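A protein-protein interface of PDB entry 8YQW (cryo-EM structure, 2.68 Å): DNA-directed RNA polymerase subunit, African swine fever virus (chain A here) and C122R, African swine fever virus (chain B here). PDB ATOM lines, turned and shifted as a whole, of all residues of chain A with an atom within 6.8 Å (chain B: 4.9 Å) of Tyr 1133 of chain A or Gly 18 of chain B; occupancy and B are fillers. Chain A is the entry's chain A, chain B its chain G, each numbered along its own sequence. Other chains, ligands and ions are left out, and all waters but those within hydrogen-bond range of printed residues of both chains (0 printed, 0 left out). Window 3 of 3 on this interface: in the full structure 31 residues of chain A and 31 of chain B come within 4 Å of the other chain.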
ATOM      1  N   LEU A1131      29.473  27.790   9.921  1.00  0.00           N
ATOM      2  CA  LEU A1131      28.206  27.598   9.228  1.00  0.00           C
ATOM      3  C   LEU A1131      27.382  26.575  10.000  1.00  0.00           C
ATOM      4  O   LEU A1131      27.758  25.402  10.076  1.00  0.00           O
ATOM      5  CB  LEU A1131      28.431  27.140   7.789  1.00  0.00           C
ATOM      6  CG  LEU A1131      27.177  26.931   6.939  1.00  0.00           C
ATOM      7  CD1 LEU A1131      26.258  28.130   7.028  1.00  0.00           C
ATOM      8  CD2 LEU A1131      27.556  26.656   5.502  1.00  0.00           C
ATOM      9  N   LEU A1132      26.262  27.019  10.564  1.00  0.00           N
ATOM     10  CA  LEU A1132      25.443  26.199  11.441  1.00  0.00           C
ATOM     11  C   LEU A1132      24.103  25.891  10.787  1.00  0.00           C
ATOM     12  O   LEU A1132      23.520  26.742  10.110  1.00  0.00           O
ATOM     13  CB  LEU A1132      25.209  26.896  12.784  1.00  0.00           C
ATOM     14  CG  LEU A1132      26.434  27.505  13.464  1.00  0.00           C
ATOM     15  CD1 LEU A1132      26.018  28.334  14.663  1.00  0.00           C
ATOM     16  CD2 LEU A1132      27.403  26.416  13.878  1.00  0.00           C
ATOM     17  N   TYR A1133      23.621  24.667  10.998  1.00  0.00           N
ATOM     18  CA  TYR A1133      22.309  24.246  10.509  1.00  0.00           C
ATOM     19  C   TYR A1133      21.261  24.527  11.587  1.00  0.00           C
ATOM     20  O   TYR A1133      20.760  23.635  12.272  1.00  0.00           O
ATOM     21  CB  TYR A1133      22.340  22.775  10.118  1.00  0.00           C
ATOM     22  CG  TYR A1133      21.176  22.334   9.261  1.00  0.00           C
ATOM     23  CD1 TYR A1133      21.121  22.658   7.914  1.00  0.00           C
ATOM     24  CD2 TYR A1133      20.140  21.579   9.797  1.00  0.00           C
ATOM     25  CE1 TYR A1133      20.062  22.257   7.128  1.00  0.00           C
ATOM     26  CE2 TYR A1133      19.079  21.171   9.016  1.00  0.00           C
ATOM     27  CZ  TYR A1133      19.045  21.514   7.682  1.00  0.00           C
ATOM     28  OH  TYR A1133      17.991  21.114   6.896  1.00  0.00           O
ATOM     29  N   GLU A1134      20.940  25.810  11.733  1.00  0.00           N
ATOM     30  CA  GLU A1134      20.025  26.260  12.771  1.00  0.00           C
ATOM     31  C   GLU A1134      19.024  27.252  12.196  1.00  0.00           C
ATOM     32  O   GLU A1134      19.299  27.941  11.212  1.00  0.00           O
ATOM     33  CB  GLU A1134      20.770  26.911  13.941  1.00  0.00           C
ATOM     34  CG  GLU A1134      21.806  26.025  14.598  1.00  0.00           C
ATOM     35  CD  GLU A1134      22.505  26.715  15.749  1.00  0.00           C
ATOM     36  OE1 GLU A1134      22.107  27.847  16.092  1.00  0.00           O
ATOM     37  OE2 GLU A1134      23.453  26.128  16.309  1.00  0.00           O
ATOM     38  N   THR A1135      17.858  27.309  12.828  1.00  0.00           N
ATOM     39  CA  THR A1135      16.828  28.291  12.531  1.00  0.00           C
ATOM     40  C   THR A1135      16.545  29.091  13.794  1.00  0.00           C
ATOM     41  O   THR A1135      16.724  28.602  14.912  1.00  0.00           O
ATOM     42  CB  THR A1135      15.540  27.618  12.041  1.00  0.00           C
ATOM     43  OG1 THR A1135      15.863  26.595  11.097  1.00  0.00           O
ATOM     44  CG2 THR A1135      14.630  28.627  11.362  1.00  0.00           C
ATOM     45  N   VAL A1143      16.842  24.032  18.382  1.00  0.00           N
ATOM     46  CA  VAL A1143      18.104  23.419  18.774  1.00  0.00           C
ATOM     47  C   VAL A1143      19.267  24.309  18.348  1.00  0.00           C
ATOM     48  O   VAL A1143      19.218  24.990  17.315  1.00  0.00           O
ATOM     49  CB  VAL A1143      18.218  22.004  18.174  1.00  0.00           C
ATOM     50  CG1 VAL A1143      18.219  22.064  16.656  1.00  0.00           C
ATOM     51  CG2 VAL A1143      19.459  21.289  18.693  1.00  0.00           C
ATOM     52  N   ASN A1173      16.843  27.055   7.507  1.00  0.00           N
ATOM     53  CA  ASN A1173      17.584  26.309   8.522  1.00  0.00           C
ATOM     54  C   ASN A1173      19.086  26.368   8.266  1.00  0.00           C
ATOM     55  O   ASN A1173      19.768  25.350   8.208  1.00  0.00           O
ATOM     56  CB  ASN A1173      17.083  24.870   8.568  1.00  0.00           C
ATOM     57  CG  ASN A1173      17.311  24.215   9.914  1.00  0.00           C
ATOM     58  OD1 ASN A1173      17.927  24.796  10.804  1.00  0.00           O
ATOM     59  ND2 ASN A1173      16.789  23.008  10.080  1.00  0.00           N
ATOM     60  N   TRP A1174      19.611  27.582   8.111  1.00  0.00           N
ATOM     61  CA  TRP A1174      21.033  27.778   7.850  1.00  0.00           C
ATOM     62  C   TRP A1174      21.480  29.063   8.523  1.00  0.00           C
ATOM     63  O   TRP A1174      20.873  30.117   8.314  1.00  0.00           O
ATOM     64  CB  TRP A1174      21.317  27.832   6.351  1.00  0.00           C
ATOM     65  CG  TRP A1174      21.072  26.542   5.651  1.00  0.00           C
ATOM     66  CD1 TRP A1174      19.937  26.166   5.000  1.00  0.00           C
ATOM     67  CD2 TRP A1174      21.989  25.453   5.521  1.00  0.00           C
ATOM     68  NE1 TRP A1174      20.088  24.908   4.474  1.00  0.00           N
ATOM     69  CE2 TRP A1174      21.340  24.447   4.781  1.00  0.00           C
ATOM     70  CE3 TRP A1174      23.296  25.229   5.961  1.00  0.00           C
ATOM     71  CZ2 TRP A1174      21.954  23.238   4.470  1.00  0.00           C
ATOM     72  CZ3 TRP A1174      23.903  24.028   5.651  1.00  0.00           C
ATOM     73  CH2 TRP A1174      23.232  23.047   4.915  1.00  0.00           C
ATOM     74  N   CYS A1175      22.541  28.976   9.318  1.00  0.00           N
ATOM     75  CA  CYS A1175      23.029  30.102  10.095  1.00  0.00           C
ATOM     76  C   CYS A1175      24.540  30.214   9.955  1.00  0.00           C
ATOM     77  O   CYS A1175      25.251  29.208   9.881  1.00  0.00           O
ATOM     78  CB  CYS A1175      22.642  29.957  11.566  1.00  0.00           C
ATOM     79  SG  CYS A1175      23.422  31.135  12.660  1.00  0.00           S
ATOM     80  N   ASP A1243      21.049  22.338  -0.871  1.00  0.00           N
ATOM     81  CA  ASP A1243      20.892  23.485   0.018  1.00  0.00           C
ATOM     82  C   ASP A1243      22.191  23.828   0.730  1.00  0.00           C
ATOM     83  O   ASP A1243      22.443  25.000   1.032  1.00  0.00           O
ATOM     84  CB  ASP A1243      19.789  23.213   1.040  1.00  0.00           C
ATOM     85  CG  ASP A1243      18.412  23.572   0.524  1.00  0.00           C
ATOM     86  OD1 ASP A1243      18.233  23.625  -0.710  1.00  0.00           O
ATOM     87  OD2 ASP A1243      17.508  23.803   1.355  1.00  0.00           O
ATOM     88  N   TYR B  15      20.250  16.257   4.632  1.00  0.00           N
ATOM     89  CA  TYR B  15      19.311  17.138   5.315  1.00  0.00           C
ATOM     90  C   TYR B  15      17.904  16.860   4.808  1.00  0.00           C
ATOM     91  O   TYR B  15      17.635  16.990   3.610  1.00  0.00           O
ATOM     92  CB  TYR B  15      19.693  18.602   5.097  1.00  0.00           C
ATOM     93  CG  TYR B  15      21.152  18.878   5.370  1.00  0.00           C
ATOM     94  CD1 TYR B  15      21.599  19.145   6.656  1.00  0.00           C
ATOM     95  CD2 TYR B  15      22.085  18.855   4.344  1.00  0.00           C
ATOM     96  CE1 TYR B  15      22.933  19.393   6.909  1.00  0.00           C
ATOM     97  CE2 TYR B  15      23.421  19.099   4.590  1.00  0.00           C
ATOM     98  CZ  TYR B  15      23.838  19.367   5.873  1.00  0.00           C
ATOM     99  OH  TYR B  15      25.167  19.613   6.121  1.00  0.00           O
ATOM    100  N   VAL B  16      17.011  16.481   5.721  1.00  0.00           N
ATOM    101  CA  VAL B  16      15.637  16.125   5.389  1.00  0.00           C
ATOM    102  C   VAL B  16      14.697  16.874   6.324  1.00  0.00           C
ATOM    103  O   VAL B  16      14.832  16.774   7.548  1.00  0.00           O
ATOM    104  CB  VAL B  16      15.400  14.606   5.489  1.00  0.00           C
ATOM    105  CG1 VAL B  16      13.917  14.291   5.398  1.00  0.00           C
ATOM    106  CG2 VAL B  16      16.169  13.879   4.396  1.00  0.00           C
ATOM    107  N   ASP B  17      13.748  17.607   5.738  1.00  0.00           N
ATOM    108  CA  ASP B  17      12.719  18.386   6.442  1.00  0.00           C
ATOM    109  C   ASP B  17      13.266  19.093   7.683  1.00  0.00           C
ATOM    110  O   ASP B  17      12.664  19.087   8.759  1.00  0.00           O
ATOM    111  CB  ASP B  17      11.492  17.520   6.774  1.00  0.00           C
ATOM    112  CG  ASP B  17      11.811  16.308   7.646  1.00  0.00           C
ATOM    113  OD1 ASP B  17      12.472  16.450   8.694  1.00  0.00           O
ATOM    114  OD2 ASP B  17      11.377  15.196   7.279  1.00  0.00           O
ATOM    115  N   GLY B  18      14.408  19.751   7.509  1.00  0.00           N
ATOM    116  CA  GLY B  18      14.994  20.520   8.589  1.00  0.00           C
ATOM    117  C   GLY B  18      15.650  19.701   9.677  1.00  0.00           C
ATOM    118  O   GLY B  18      15.629  20.104  10.843  1.00  0.00           O
ATOM    119  N   ASN B  19      16.232  18.557   9.328  1.00  0.00           N
ATOM    120  CA  ASN B  19      16.930  17.717  10.287  1.00  0.00           C
ATOM    121  C   ASN B  19      18.118  17.068   9.593  1.00  0.00           C
ATOM    122  O   ASN B  19      18.089  16.823   8.385  1.00  0.00           O
ATOM    123  CB  ASN B  19      16.008  16.647  10.879  1.00  0.00           C
ATOM    124  CG  ASN B  19      16.276  16.395  12.347  1.00  0.00           C
ATOM    125  OD1 ASN B  19      16.665  17.303  13.081  1.00  0.00           O
ATOM    126  ND2 ASN B  19      16.072  15.160  12.784  1.00  0.00           N
ATOM    127  N   ILE B  20      19.161  16.791  10.368  1.00  0.00           N
ATOM    128  CA  ILE B  20      20.379  16.177   9.857  1.00  0.00           C
ATOM    129  C   ILE B  20      20.276  14.671  10.041  1.00  0.00           C
ATOM    130  O   ILE B  20      20.009  14.191  11.150  1.00  0.00           O
ATOM    131  CB  ILE B  20      21.627  16.737  10.560  1.00  0.00           C
ATOM    132  CG1 ILE B  20      21.932  18.145  10.057  1.00  0.00           C
ATOM    133  CG2 ILE B  20      22.821  15.834  10.327  1.00  0.00           C
ATOM    134  CD1 ILE B  20      23.007  18.853  10.841  1.00  0.00           C
ATOM    135  N   LEU B  37      25.335  20.038  14.376  1.00  0.00           N
ATOM    136  CA  LEU B  37      24.879  21.231  13.663  1.00  0.00           C
ATOM    137  C   LEU B  37      26.031  22.191  13.386  1.00  0.00           C
ATOM    138  O   LEU B  37      25.958  23.381  13.681  1.00  0.00           O
ATOM    139  CB  LEU B  37      23.778  21.922  14.456  1.00  0.00           C
ATOM    140  CG  LEU B  37      22.607  21.063  14.923  1.00  0.00           C
ATOM    141  CD1 LEU B  37      21.804  21.812  15.967  1.00  0.00           C
ATOM    142  CD2 LEU B  37      21.732  20.670  13.750  1.00  0.00           C
ATOM    143  N   VAL B  39      28.096  22.682   9.994  1.00  0.00           N
ATOM    144  CA  VAL B  39      28.311  22.261   8.615  1.00  0.00           C
ATOM    145  C   VAL B  39      29.753  22.517   8.195  1.00  0.00           C
ATOM    146  O   VAL B  39      30.404  21.653   7.600  1.00  0.00           O
ATOM    147  CB  VAL B  39      27.314  22.970   7.684  1.00  0.00           C
ATOM    148  CG1 VAL B  39      27.312  22.312   6.319  1.00  0.00           C
ATOM    149  CG2 VAL B  39      25.928  22.956   8.301  1.00  0.00           C
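CD2 of Leu 1132 of chain A touches O of Leu 37 of chain B, at 3.4 Å.
Tyr 15 of chain B touches Tyr 1133 of chain A.
OH of Tyr 1133 of chain A touches CA of Gly 18 of chain B (3.5 Å).
CE2 of Tyr 1133 of chain A touches N of Asn 19 of chain B (3.9 Å).
CG1 of Ile 20 of chain B touches CD2 of Tyr 1133 of chain A, at 3.9 Å.
Leu 37 of chain B touches Tyr 1133 of chain A.
Val 39 of chain B touches Tyr 1133 of chain A (CG2 to N, 3.9 Å).
Leu 37 of chain B touches Val 1143 of chain A.
Trp 1174 of chain A touches Tyr 15 of chain B (CH2 to CZ, 3.9 Å).
CZ3 of Trp 1174 of chain A touches CG2 of Val 39 of chain B, at 3.5 Å.
O of Leu 1131 of chain A sits at hydrogen-bond distance from N of Val 39 of chain B (2.7 Å).
ND2 of Asn 1173 of chain A lies within hydrogen-bond range of O of Gly 18 of chain B (3.2 Å).
Printed residues of chain B within 4 Å of Leu 1131 of chain A: Val 39.
Printed residues of chain B within 4 Å of Val 1143 of chain A: Leu 37.
Of the printed residues of chain B, Asn 1173 of chain A touches Gly 18 (3.2 Å).
Printed residues of chain B within 4 Å of Trp 1174 of chain A: Tyr 15 and Val 39.
The nearest printed residue of chain B that does not touch Tyr 1133 of chain A is Val 16 of chain B (4.9 Å).
The nearest residue of chain A that does not touch Gly 18 of chain B is Thr 1135 of chain A (6.5 Å).
The side-chain amide oxygen (OD1) of Asn 1173 of chain A is in hydrogen-bond range of the side-chain hydroxyl (OG1) of Thr 1135 of chain A.
OD1 of Asn 1173 of chain A sits close to N of Glu 1134 of chain A (3.3 Å).
O of Glu 1134 of chain A is in hydrogen-bond range of N of Trp 1174 of chain A, 3.1 Å away.
The backbone NH (N) of Leu 1132 of chain A sits at hydrogen-bond distance from the backbone carbonyl oxygen (O) of Cys 1175 of chain A, 2.5 Å away.
The backbone carbonyl oxygen (O) of Tyr 1133 of chain A sits close to the side-chain amide oxygen (OD1) of Asn 1173 of chain A (3.4 Å).
Of the 8 printed residues of chain B, 6 touch a printed residue of chain A.
Printed residues of chain B that touch a printed residue of chain A: Tyr 15, Gly 18, Asn 19, Ile 20, Leu 37 and Val 39.
Of the 10 printed residues of chain A, 6 touch a printed residue of chain B.
Hydrophobic or aromatic side chains of chain A that line the printed part of chain B: Leu 1132, Tyr 1133, Val 1143 and Trp 1174.
Among the printed residues, 12 pairs touch across the chains.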
